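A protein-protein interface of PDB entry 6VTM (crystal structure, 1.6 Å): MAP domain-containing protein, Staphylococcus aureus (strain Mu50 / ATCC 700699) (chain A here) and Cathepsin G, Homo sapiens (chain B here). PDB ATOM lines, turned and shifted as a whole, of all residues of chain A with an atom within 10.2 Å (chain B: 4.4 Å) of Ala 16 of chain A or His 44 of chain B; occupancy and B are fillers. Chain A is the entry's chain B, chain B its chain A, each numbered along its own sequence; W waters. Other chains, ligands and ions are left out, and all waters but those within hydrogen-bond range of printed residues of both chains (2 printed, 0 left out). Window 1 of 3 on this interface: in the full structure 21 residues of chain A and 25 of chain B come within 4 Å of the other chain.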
ATOM      1  N   TYR A   7      -8.155  14.942 -17.647  1.00  0.00           N
ATOM      2  CA  TYR A   7      -6.879  15.039 -18.341  1.00  0.00           C
ATOM      3  C   TYR A   7      -6.882  14.139 -19.552  1.00  0.00           C
ATOM      4  O   TYR A   7      -7.683  13.199 -19.640  1.00  0.00           O
ATOM      5  CB  TYR A   7      -5.714  14.690 -17.438  1.00  0.00           C
ATOM      6  CG  TYR A   7      -5.687  13.292 -16.966  1.00  0.00           C
ATOM      7  CD1 TYR A   7      -6.439  12.891 -15.859  1.00  0.00           C
ATOM      8  CD2 TYR A   7      -4.948  12.327 -17.645  1.00  0.00           C
ATOM      9  CE1 TYR A   7      -6.418  11.553 -15.415  1.00  0.00           C
ATOM     10  CE2 TYR A   7      -4.898  10.995 -17.198  1.00  0.00           C
ATOM     11  CZ  TYR A   7      -5.637  10.617 -16.077  1.00  0.00           C
ATOM     12  OH  TYR A   7      -5.610   9.312 -15.633  1.00  0.00           O
ATOM     13  N   THR A   8      -5.976  14.435 -20.478  1.00  0.00           N
ATOM     14  CA  THR A   8      -5.857  13.691 -21.726  1.00  0.00           C
ATOM     15  C   THR A   8      -4.404  13.301 -21.918  1.00  0.00           C
ATOM     16  O   THR A   8      -3.498  14.073 -21.606  1.00  0.00           O
ATOM     17  CB  THR A   8      -6.328  14.511 -22.941  1.00  0.00           C
ATOM     18  OG1 THR A   8      -7.712  14.870 -22.780  1.00  0.00           O
ATOM     19  CG2 THR A   8      -6.156  13.707 -24.230  1.00  0.00           C
ATOM     20  N   ILE A   9      -4.169  12.099 -22.423  1.00  0.00           N
ATOM     21  CA  ILE A   9      -2.825  11.613 -22.694  1.00  0.00           C
ATOM     22  C   ILE A   9      -2.694  11.349 -24.175  1.00  0.00           C
ATOM     23  O   ILE A   9      -3.492  10.591 -24.743  1.00  0.00           O
ATOM     24  CB  ILE A   9      -2.493  10.333 -21.914  1.00  0.00           C
ATOM     25  CG1 ILE A   9      -2.344  10.683 -20.436  1.00  0.00           C
ATOM     26  CG2 ILE A   9      -1.188   9.753 -22.434  1.00  0.00           C
ATOM     27  CD1 ILE A   9      -2.214   9.470 -19.559  1.00  0.00           C
ATOM     28  N   SER A  10      -1.679  11.948 -24.783  1.00  0.00           N
ATOM     29  CA  SER A  10      -1.322  11.695 -26.174  1.00  0.00           C
ATOM     30  C   SER A  10       0.121  11.228 -26.196  1.00  0.00           C
ATOM     31  O   SER A  10       1.018  11.916 -25.689  1.00  0.00           O
ATOM     32  CB  SER A  10      -1.505  12.934 -27.038  1.00  0.00           C
ATOM     33  OG  SER A  10      -2.851  13.418 -26.988  1.00  0.00           O
ATOM     34  N   VAL A  11       0.339  10.046 -26.740  1.00  0.00           N
ATOM     35  CA  VAL A  11       1.678   9.501 -26.860  1.00  0.00           C
ATOM     36  C   VAL A  11       1.878   9.044 -28.296  1.00  0.00           C
ATOM     37  O   VAL A  11       1.090   8.239 -28.799  1.00  0.00           O
ATOM     38  CB  VAL A  11       1.915   8.342 -25.886  1.00  0.00           C
ATOM     39  CG1 VAL A  11       3.271   7.696 -26.163  1.00  0.00           C
ATOM     40  CG2 VAL A  11       1.804   8.821 -24.452  1.00  0.00           C
ATOM     41  N   ASP A  12       2.942   9.534 -28.939  1.00  0.00           N
ATOM     42  CA  ASP A  12       3.280   9.146 -30.318  1.00  0.00           C
ATOM     43  C   ASP A  12       2.122   9.430 -31.269  1.00  0.00           C
ATOM     44  O   ASP A  12       1.909   8.692 -32.238  1.00  0.00           O
ATOM     45  CB  ASP A  12       3.697   7.672 -30.400  1.00  0.00           C
ATOM     46  CG  ASP A  12       4.982   7.383 -29.631  1.00  0.00           C
ATOM     47  OD1 ASP A  12       5.816   8.303 -29.478  1.00  0.00           O
ATOM     48  OD2 ASP A  12       5.149   6.233 -29.174  1.00  0.00           O
ATOM     49  N   GLY A  13       1.381  10.504 -30.990  1.00  0.00           N
ATOM     50  CA  GLY A  13       0.285  10.940 -31.825  1.00  0.00           C
ATOM     51  C   GLY A  13      -1.019  10.208 -31.632  1.00  0.00           C
ATOM     52  O   GLY A  13      -1.956  10.446 -32.403  1.00  0.00           O
ATOM     53  N   ILE A  14      -1.098   9.289 -30.668  1.00  0.00           N
ATOM     54  CA  ILE A  14      -2.280   8.485 -30.408  1.00  0.00           C
ATOM     55  C   ILE A  14      -2.863   8.908 -29.070  1.00  0.00           C
ATOM     56  O   ILE A  14      -2.133   8.993 -28.068  1.00  0.00           O
ATOM     57  CB  ILE A  14      -1.940   6.979 -30.356  1.00  0.00           C
ATOM     58  CG1 ILE A  14      -1.564   6.472 -31.738  1.00  0.00           C
ATOM     59  CG2 ILE A  14      -3.078   6.146 -29.703  1.00  0.00           C
ATOM     60  CD1 ILE A  14      -1.039   5.042 -31.710  1.00  0.00           C
ATOM     61  N   THR A  15      -4.170   9.142 -29.056  1.00  0.00           N
ATOM     62  CA  THR A  15      -4.956   9.383 -27.845  1.00  0.00           C
ATOM     63  C   THR A  15      -6.035   8.313 -27.710  1.00  0.00           C
ATOM     64  O   THR A  15      -6.958   8.255 -28.523  1.00  0.00           O
ATOM     65  CB  THR A  15      -5.581  10.775 -27.892  1.00  0.00           C
ATOM     66  OG1 THR A  15      -4.520  11.740 -28.033  1.00  0.00           O
ATOM     67  CG2 THR A  15      -6.379  11.057 -26.637  1.00  0.00           C
ATOM     68  N   ALA A  16      -5.949   7.490 -26.660  1.00  0.00           N
ATOM     69  CA  ALA A  16      -7.046   6.579 -26.345  1.00  0.00           C
ATOM     70  C   ALA A  16      -8.294   7.382 -25.991  1.00  0.00           C
ATOM     71  O   ALA A  16      -8.210   8.455 -25.383  1.00  0.00           O
ATOM     72  CB  ALA A  16      -6.674   5.661 -25.193  1.00  0.00           C
ATOM     73  N   LEU A  17      -9.464   6.878 -26.372  1.00  0.00           N
ATOM     74  CA  LEU A  17     -10.682   7.683 -26.325  1.00  0.00           C
ATOM     75  C   LEU A  17     -11.573   7.385 -25.117  1.00  0.00           C
ATOM     76  O   LEU A  17     -12.790   7.651 -25.167  1.00  0.00           O
ATOM     77  CB  LEU A  17     -11.444   7.555 -27.655  1.00  0.00           C
ATOM     78  CG  LEU A  17     -10.727   8.212 -28.852  1.00  0.00           C
ATOM     79  CD1 LEU A  17     -11.445   7.893 -30.133  1.00  0.00           C
ATOM     80  CD2 LEU A  17     -10.618   9.735 -28.647  1.00  0.00           C
ATOM     81  N   HIS A  18     -10.994   6.914 -24.006  1.00  0.00           N
ATOM     82  CA  HIS A  18     -11.687   6.990 -22.723  1.00  0.00           C
ATOM     83  C   HIS A  18     -11.687   8.429 -22.227  1.00  0.00           C
ATOM     84  O   HIS A  18     -11.031   9.307 -22.794  1.00  0.00           O
ATOM     85  CB  HIS A  18     -11.075   6.072 -21.681  1.00  0.00           C
ATOM     86  CG  HIS A  18      -9.599   6.201 -21.452  1.00  0.00           C
ATOM     87  ND1 HIS A  18      -8.770   7.062 -22.135  1.00  0.00           N
ATOM     88  CD2 HIS A  18      -8.804   5.522 -20.588  1.00  0.00           C
ATOM     89  CE1 HIS A  18      -7.525   6.902 -21.699  1.00  0.00           C
ATOM     90  NE2 HIS A  18      -7.522   5.960 -20.784  1.00  0.00           N
ATOM     91  N   ARG A  19     -12.469   8.687 -21.177  1.00  0.00           N
ATOM     92  CA  ARG A  19     -12.448   9.986 -20.517  1.00  0.00           C
ATOM     93  C   ARG A  19     -11.863   9.731 -19.138  1.00  0.00           C
ATOM     94  O   ARG A  19     -12.406   8.925 -18.372  1.00  0.00           O
ATOM     95  CB  ARG A  19     -13.855  10.571 -20.437  1.00  0.00           C
ATOM     96  CG  ARG A  19     -13.993  11.869 -19.668  1.00  0.00           C
ATOM     97  CD  ARG A  19     -13.188  12.951 -20.298  1.00  0.00           C
ATOM     98  NE  ARG A  19     -13.629  14.283 -19.878  1.00  0.00           N
ATOM     99  CZ  ARG A  19     -13.063  15.413 -20.285  1.00  0.00           C
ATOM    100  NH1 ARG A  19     -12.015  15.375 -21.099  1.00  0.00           N
ATOM    101  NH2 ARG A  19     -13.532  16.576 -19.864  1.00  0.00           N
ATOM    102  N   THR A  20     -10.723  10.357 -18.840  1.00  0.00           N
ATOM    103  CA  THR A  20     -10.014  10.164 -17.580  1.00  0.00           C
ATOM    104  C   THR A  20      -9.989  11.442 -16.740  1.00  0.00           C
ATOM    105  O   THR A  20      -9.856  12.534 -17.277  1.00  0.00           O
ATOM    106  CB  THR A  20      -8.565   9.705 -17.836  1.00  0.00           C
ATOM    107  OG1 THR A  20      -7.952  10.507 -18.827  1.00  0.00           O
ATOM    108  CG2 THR A  20      -8.571   8.254 -18.337  1.00  0.00           C
ATOM    109  N   GLU A  42       0.569   7.907 -14.761  1.00  0.00           N
ATOM    110  CA  GLU A  42      -0.466   7.580 -15.745  1.00  0.00           C
ATOM    111  C   GLU A  42       0.143   7.303 -17.117  1.00  0.00           C
ATOM    112  O   GLU A  42      -0.313   6.400 -17.834  1.00  0.00           O
ATOM    113  CB  GLU A  42      -1.513   8.686 -15.863  1.00  0.00           C
ATOM    114  CG  GLU A  42      -2.374   8.861 -14.604  1.00  0.00           C
ATOM    115  CD  GLU A  42      -3.040   7.570 -14.120  1.00  0.00           C
ATOM    116  OE1 GLU A  42      -3.513   6.793 -14.963  1.00  0.00           O
ATOM    117  OE2 GLU A  42      -3.151   7.332 -12.894  1.00  0.00           O
ATOM    118  N   SER A  45       1.207   3.691 -16.588  1.00  0.00           N
ATOM    119  CA  SER A  45       0.179   2.679 -16.416  1.00  0.00           C
ATOM    120  C   SER A  45      -0.835   2.645 -17.546  1.00  0.00           C
ATOM    121  O   SER A  45      -1.457   1.597 -17.765  1.00  0.00           O
ATOM    122  CB  SER A  45      -0.582   2.896 -15.115  1.00  0.00           C
ATOM    123  OG  SER A  45      -1.314   4.103 -15.160  1.00  0.00           O
ATOM    124  N   GLN A  46      -1.037   3.748 -18.255  1.00  0.00           N
ATOM    125  CA  GLN A  46      -1.963   3.741 -19.382  1.00  0.00           C
ATOM    126  C   GLN A  46      -1.289   3.422 -20.712  1.00  0.00           C
ATOM    127  O   GLN A  46      -1.887   2.765 -21.575  1.00  0.00           O
ATOM    128  CB  GLN A  46      -2.656   5.098 -19.525  1.00  0.00           C
ATOM    129  CG  GLN A  46      -3.577   5.379 -18.351  1.00  0.00           C
ATOM    130  CD  GLN A  46      -4.377   6.650 -18.488  1.00  0.00           C
ATOM    131  OE1 GLN A  46      -4.678   7.121 -19.586  1.00  0.00           O
ATOM    132  NE2 GLN A  46      -4.737   7.220 -17.351  1.00  0.00           N
ATOM    133  N   ARG A  47      -0.063   3.884 -20.930  1.00  0.00           N
ATOM    134  CA  ARG A  47       0.556   3.806 -22.254  1.00  0.00           C
ATOM    135  C   ARG A  47       1.964   3.241 -22.218  1.00  0.00           C
ATOM    136  O   ARG A  47       2.649   3.248 -23.248  1.00  0.00           O
ATOM    137  CB  ARG A  47       0.558   5.199 -22.917  1.00  0.00           C
ATOM    138  CG  ARG A  47      -0.839   5.711 -23.281  1.00  0.00           C
ATOM    139  CD  ARG A  47      -1.560   4.849 -24.335  1.00  0.00           C
ATOM    140  NE  ARG A  47      -0.764   4.728 -25.550  1.00  0.00           N
ATOM    141  CZ  ARG A  47      -0.678   5.668 -26.479  1.00  0.00           C
ATOM    142  NH1 ARG A  47      -1.379   6.789 -26.377  1.00  0.00           N
ATOM    143  NH2 ARG A  47       0.109   5.495 -27.524  1.00  0.00           N
ATOM    144  N   GLY A  48       2.405   2.704 -21.086  1.00  0.00           N
ATOM    145  CA  GLY A  48       3.675   2.014 -21.066  1.00  0.00           C
ATOM    146  C   GLY A  48       4.883   2.898 -21.287  1.00  0.00           C
ATOM    147  O   GLY A  48       5.932   2.413 -21.736  1.00  0.00           O
ATOM    148  N   GLN A  95      -3.464  18.632 -20.086  1.00  0.00           N
ATOM    149  CA  GLN A  95      -3.160  18.030 -21.376  1.00  0.00           C
ATOM    150  C   GLN A  95      -1.740  17.488 -21.329  1.00  0.00           C
ATOM    151  O   GLN A  95      -0.797  18.249 -21.109  1.00  0.00           O
ATOM    152  CB  GLN A  95      -3.299  19.069 -22.495  1.00  0.00           C
ATOM    153  CG  GLN A  95      -3.218  18.506 -23.888  1.00  0.00           C
ATOM    154  CD  GLN A  95      -4.562  18.036 -24.420  1.00  0.00           C
ATOM    155  OE1 GLN A  95      -5.593  18.107 -23.739  1.00  0.00           O
ATOM    156  NE2 GLN A  95      -4.558  17.572 -25.659  1.00  0.00           N
ATOM    157  N   ILE A  96      -1.580  16.189 -21.547  1.00  0.00           N
ATOM    158  CA  ILE A  96      -0.289  15.520 -21.455  1.00  0.00           C
ATOM    159  C   ILE A  96       0.118  15.068 -22.853  1.00  0.00           C
ATOM    160  O   ILE A  96      -0.646  14.347 -23.508  1.00  0.00           O
ATOM    161  CB  ILE A  96      -0.359  14.323 -20.490  1.00  0.00           C
ATOM    162  CG1 ILE A  96      -0.772  14.780 -19.075  1.00  0.00           C
ATOM    163  CG2 ILE A  96       0.953  13.624 -20.402  1.00  0.00           C
ATOM    164  CD1 ILE A  96      -1.427  13.689 -18.255  1.00  0.00           C
ATOM    165  N   ALA B  42     -13.209  -1.808 -24.531  1.00  0.00           N
ATOM    166  CA  ALA B  42     -11.794  -1.670 -24.854  1.00  0.00           C
ATOM    167  C   ALA B  42     -10.925  -2.035 -23.656  1.00  0.00           C
ATOM    168  O   ALA B  42     -11.273  -1.737 -22.508  1.00  0.00           O
ATOM    169  CB  ALA B  42     -11.504  -0.238 -25.288  1.00  0.00           C
ATOM    170  N   ALA B  43      -9.779  -2.672 -23.930  1.00  0.00           N
ATOM    171  CA  ALA B  43      -8.863  -3.058 -22.854  1.00  0.00           C
ATOM    172  C   ALA B  43      -8.248  -1.863 -22.135  1.00  0.00           C
ATOM    173  O   ALA B  43      -7.873  -1.978 -20.960  1.00  0.00           O
ATOM    174  CB  ALA B  43      -7.729  -3.927 -23.393  1.00  0.00           C
ATOM    175  N   HIS B  44      -8.113  -0.722 -22.810  1.00  0.00           N
ATOM    176  CA  HIS B  44      -7.577   0.451 -22.133  1.00  0.00           C
ATOM    177  C   HIS B  44      -8.555   1.010 -21.090  1.00  0.00           C
ATOM    178  O   HIS B  44      -8.169   1.901 -20.322  1.00  0.00           O
ATOM    179  CB  HIS B  44      -7.122   1.538 -23.168  1.00  0.00           C
ATOM    180  CG  HIS B  44      -8.229   2.328 -23.813  1.00  0.00           C
ATOM    181  ND1 HIS B  44      -8.569   2.185 -25.144  1.00  0.00           N
ATOM    182  CD2 HIS B  44      -9.036   3.301 -23.325  1.00  0.00           C
ATOM    183  CE1 HIS B  44      -9.575   2.998 -25.429  1.00  0.00           C
ATOM    184  NE2 HIS B  44      -9.856   3.710 -24.348  1.00  0.00           N
ATOM    185  N   CYS B  45      -9.769   0.466 -20.987  1.00  0.00           N
ATOM    186  CA  CYS B  45     -10.774   0.826 -19.989  1.00  0.00           C
ATOM    187  C   CYS B  45     -10.698  -0.020 -18.718  1.00  0.00           C
ATOM    188  O   CYS B  45     -11.593   0.065 -17.857  1.00  0.00           O
ATOM    189  CB  CYS B  45     -12.176   0.716 -20.582  1.00  0.00           C
ATOM    190  SG  CYS B  45     -12.460   1.882 -21.980  1.00  0.00           S
ATOM    191  N   TRP B  46      -9.656  -0.812 -18.560  1.00  0.00           N
ATOM    192  CA  TRP B  46      -9.527  -1.640 -17.375  1.00  0.00           C
ATOM    193  C   TRP B  46      -9.290  -0.800 -16.136  1.00  0.00           C
ATOM    194  O   TRP B  46      -8.584   0.223 -16.160  1.00  0.00           O
ATOM    195  CB  TRP B  46      -8.371  -2.579 -17.587  1.00  0.00           C
ATOM    196  CG  TRP B  46      -8.185  -3.702 -16.698  1.00  0.00           C
ATOM    197  CD1 TRP B  46      -9.053  -4.738 -16.459  1.00  0.00           C
ATOM    198  CD2 TRP B  46      -6.972  -4.029 -16.038  1.00  0.00           C
ATOM    199  NE1 TRP B  46      -8.461  -5.663 -15.638  1.00  0.00           N
ATOM    200  CE2 TRP B  46      -7.176  -5.253 -15.374  1.00  0.00           C
ATOM    201  CE3 TRP B  46      -5.729  -3.391 -15.926  1.00  0.00           C
ATOM    202  CZ2 TRP B  46      -6.185  -5.849 -14.602  1.00  0.00           C
ATOM    203  CZ3 TRP B  46      -4.747  -3.981 -15.156  1.00  0.00           C
ATOM    204  CH2 TRP B  46      -4.977  -5.200 -14.509  1.00  0.00           C
ATOM    205  N   TYR B  80      -2.929  -7.599 -25.466  1.00  0.00           N
ATOM    206  CA  TYR B  80      -3.121  -6.148 -25.419  1.00  0.00           C
ATOM    207  C   TYR B  80      -1.770  -5.471 -25.234  1.00  0.00           C
ATOM    208  O   TYR B  80      -0.990  -5.850 -24.354  1.00  0.00           O
ATOM    209  CB  TYR B  80      -4.078  -5.764 -24.282  1.00  0.00           C
ATOM    210  CG  TYR B  80      -4.141  -4.293 -24.024  1.00  0.00           C
ATOM    211  CD1 TYR B  80      -4.455  -3.407 -25.028  1.00  0.00           C
ATOM    212  CD2 TYR B  80      -3.872  -3.799 -22.773  1.00  0.00           C
ATOM    213  CE1 TYR B  80      -4.490  -2.025 -24.773  1.00  0.00           C
ATOM    214  CE2 TYR B  80      -3.919  -2.457 -22.512  1.00  0.00           C
ATOM    215  CZ  TYR B  80      -4.250  -1.576 -23.495  1.00  0.00           C
ATOM    216  OH  TYR B  80      -4.281  -0.230 -23.188  1.00  0.00           O
ATOM    217  N   ILE B  85      -1.526   0.467 -28.463  1.00  0.00           N
ATOM    218  CA  ILE B  85      -2.965   0.255 -28.345  1.00  0.00           C
ATOM    219  C   ILE B  85      -3.353  -0.750 -29.419  1.00  0.00           C
ATOM    220  O   ILE B  85      -4.216  -0.495 -30.271  1.00  0.00           O
ATOM    221  CB  ILE B  85      -3.766   1.555 -28.431  1.00  0.00           C
ATOM    222  CG1 ILE B  85      -3.080   2.670 -27.653  1.00  0.00           C
ATOM    223  CG2 ILE B  85      -5.152   1.321 -27.883  1.00  0.00           C
ATOM    224  CD1 ILE B  85      -3.982   3.884 -27.434  1.00  0.00           C
ATOM    225  N   ASP B  88      -6.884  -4.106 -28.535  1.00  0.00           N
ATOM    226  CA  ASP B  88      -7.588  -3.303 -27.530  1.00  0.00           C
ATOM    227  C   ASP B  88      -9.033  -3.802 -27.425  1.00  0.00           C
ATOM    228  O   ASP B  88      -9.977  -3.239 -27.995  1.00  0.00           O
ATOM    229  CB  ASP B  88      -7.523  -1.833 -27.928  1.00  0.00           C
ATOM    230  CG  ASP B  88      -8.015  -0.908 -26.857  1.00  0.00           C
ATOM    231  OD1 ASP B  88      -8.122  -1.310 -25.663  1.00  0.00           O
ATOM    232  OD2 ASP B  88      -8.321   0.280 -27.202  1.00  0.00           O
ATOM    233  N   SER B 181     -14.821   5.508 -26.072  1.00  0.00           N
ATOM    234  CA  SER B 181     -14.054   4.265 -26.119  1.00  0.00           C
ATOM    235  C   SER B 181     -14.853   3.098 -25.588  1.00  0.00           C
ATOM    236  O   SER B 181     -15.547   3.194 -24.567  1.00  0.00           O
ATOM    237  CB  SER B 181     -12.759   4.372 -25.308  1.00  0.00           C
ATOM    238  OG  SER B 181     -11.716   4.787 -26.152  1.00  0.00           O
ATOM    239  N   SER B 196     -11.548   2.771 -30.215  1.00  0.00           N
ATOM    240  CA  SER B 196     -10.248   2.614 -29.570  1.00  0.00           C
ATOM    241  C   SER B 196      -9.529   3.946 -29.413  1.00  0.00           C
ATOM    242  O   SER B 196      -9.394   4.421 -28.281  1.00  0.00           O
ATOM    243  CB  SER B 196      -9.416   1.603 -30.366  1.00  0.00           C
ATOM    244  OG  SER B 196      -8.148   1.382 -29.752  1.00  0.00           O
ATOM    245  N   TYR B 197      -9.009   4.533 -30.498  1.00  0.00           N
ATOM    246  CA  TYR B 197      -8.186   5.715 -30.380  1.00  0.00           C
ATOM    247  C   TYR B 197      -8.259   6.616 -31.589  1.00  0.00           C
ATOM    248  O   TYR B 197      -8.742   6.248 -32.648  1.00  0.00           O
ATOM    249  CB  TYR B 197      -6.736   5.358 -30.135  1.00  0.00           C
ATOM    250  CG  TYR B 197      -5.914   4.708 -31.246  1.00  0.00           C
ATOM    251  CD1 TYR B 197      -5.391   5.448 -32.276  1.00  0.00           C
ATOM    252  CD2 TYR B 197      -5.600   3.345 -31.182  1.00  0.00           C
ATOM    253  CE1 TYR B 197      -4.563   4.863 -33.243  1.00  0.00           C
ATOM    254  CE2 TYR B 197      -4.774   2.763 -32.116  1.00  0.00           C
ATOM    255  CZ  TYR B 197      -4.295   3.507 -33.169  1.00  0.00           C
ATOM    256  OH  TYR B 197      -3.460   2.928 -34.110  1.00  0.00           O
HETATM  257  O   HOH W   1      -3.703   0.700 -20.858  1.00  0.00           O
HETATM  258  O   HOH W   2      -3.473   2.077 -24.334  1.00  0.00           O
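The side-chain hydroxyl of Ser 181 of chain B sits at hydrogen-bond distance from the backbone carbonyl oxygen of Ser 196 of chain B, at 3.2 Å. The side-chain hydroxyl (OG) of Ser 196 of chain B lies within hydrogen-bond range of the side-chain carboxylate (OD2) of Asp 88 of chain B (2.8 Å). OG of Ser 10 of chain A sits at hydrogen-bond distance from OG1 of Thr 15 of chain A, at 2.6 Å. The guanidinium group (NH2) of Arg 47 of chain A sits at hydrogen-bond distance from the backbone carbonyl oxygen (O) of Val 11 of chain A (3.2 Å). NH1 of Arg 47 of chain A sits at hydrogen-bond distance from O of Ile 14 of chain A (2.9 Å). The side-chain carboxylate of Asp 88 of chain B is in hydrogen-bond range of a ring nitrogen (ND1) of His 44 of chain B, 2.8 Å away.
NE2 of His 44 of chain B sits at hydrogen-bond distance from N of His 18 of chain A (3.4 Å). N of Leu 17 of chain A lies within hydrogen-bond range of O of Ser 196 of chain B (3.1 Å). N of His 18 of chain A sits at hydrogen-bond distance from OG of Ser 181 of chain B, 3.1 Å away. The backbone NH (N) of Leu 17 of chain A lies close to the side-chain hydroxyl (OG) of Ser 181 of chain B, 3.1 Å away.
Water W1 bridges OH of Tyr 80 of chain B (2.6 Å) and O of Gln 46 of chain A (2.8 Å). Water W2 lies within hydrogen-bond range of OH of Tyr 80 of chain B and O of Gln 46 of chain A.
Among the printed residues, pairs that only touch across the chains: Ile 14 of chain A with Ile 85 of chain B (3.3 Å), Ile 14 of chain A with Tyr 197 of chain B (3.5 Å), Thr 15 of chain A with Tyr 197 of chain B (3.3 Å), Ala 16 of chain A with His 44 of chain B (3.8 Å), Ala 16 of chain A with Ile 85 of chain B (3.9 Å), Ala 16 of chain A with Ser 196 of chain B (3.7 Å), Ala 16 of chain A with Tyr 197 of chain B (3.99 Å), Leu 17 of chain A with His 44 of chain B (3.8 Å), Leu 17 of chain A with Tyr 197 of chain B (3.7 Å) and Arg 47 of chain A with Ile 85 of chain B (3.7 Å).
Hydrophobic or aromatic side chains of chain B within 4 Å of the printed part of chain A: His 44, Ile 85 and Tyr 197. Of the 21 printed residues of chain A, 6 touch a printed residue of chain B. Hydrophobic or aromatic side chains of chain A within 4 Å of the printed part of chain B: Ile 14, Ala 16, Leu 17 and His 18. Among the printed residues, no Asp or Glu carboxylate lies within 4 Å of a Lys or Arg side-chain nitrogen of the other chain.
Printed residues of chain B within 4 Å of Ile 14 of chain A: Ile 85 (3.3 Å) and Tyr 197 (3.5 Å). Of the printed residues of chain B, Ala 16 of chain A touches His 44, Ile 85, Ser 196 and Tyr 197. Glu 42 of chain A touches none of the printed residues of chain B. Printed residues of chain B within 4 Å of Arg 47 of chain A: Ile 85. No residue of chain A comes within 4 Å of Ala 43 of chain B. His 44 of chain B touches three residues of chain A. Cys 45 of chain B touches none of the printed residues of chain A. The nearest printed residue of chain B that does not touch Ala 16 of chain A is Ser 181 of chain B (4.3 Å). The nearest printed residue of chain B that does not touch Arg 47 of chain A is Tyr 80 of chain B (5.9 Å).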
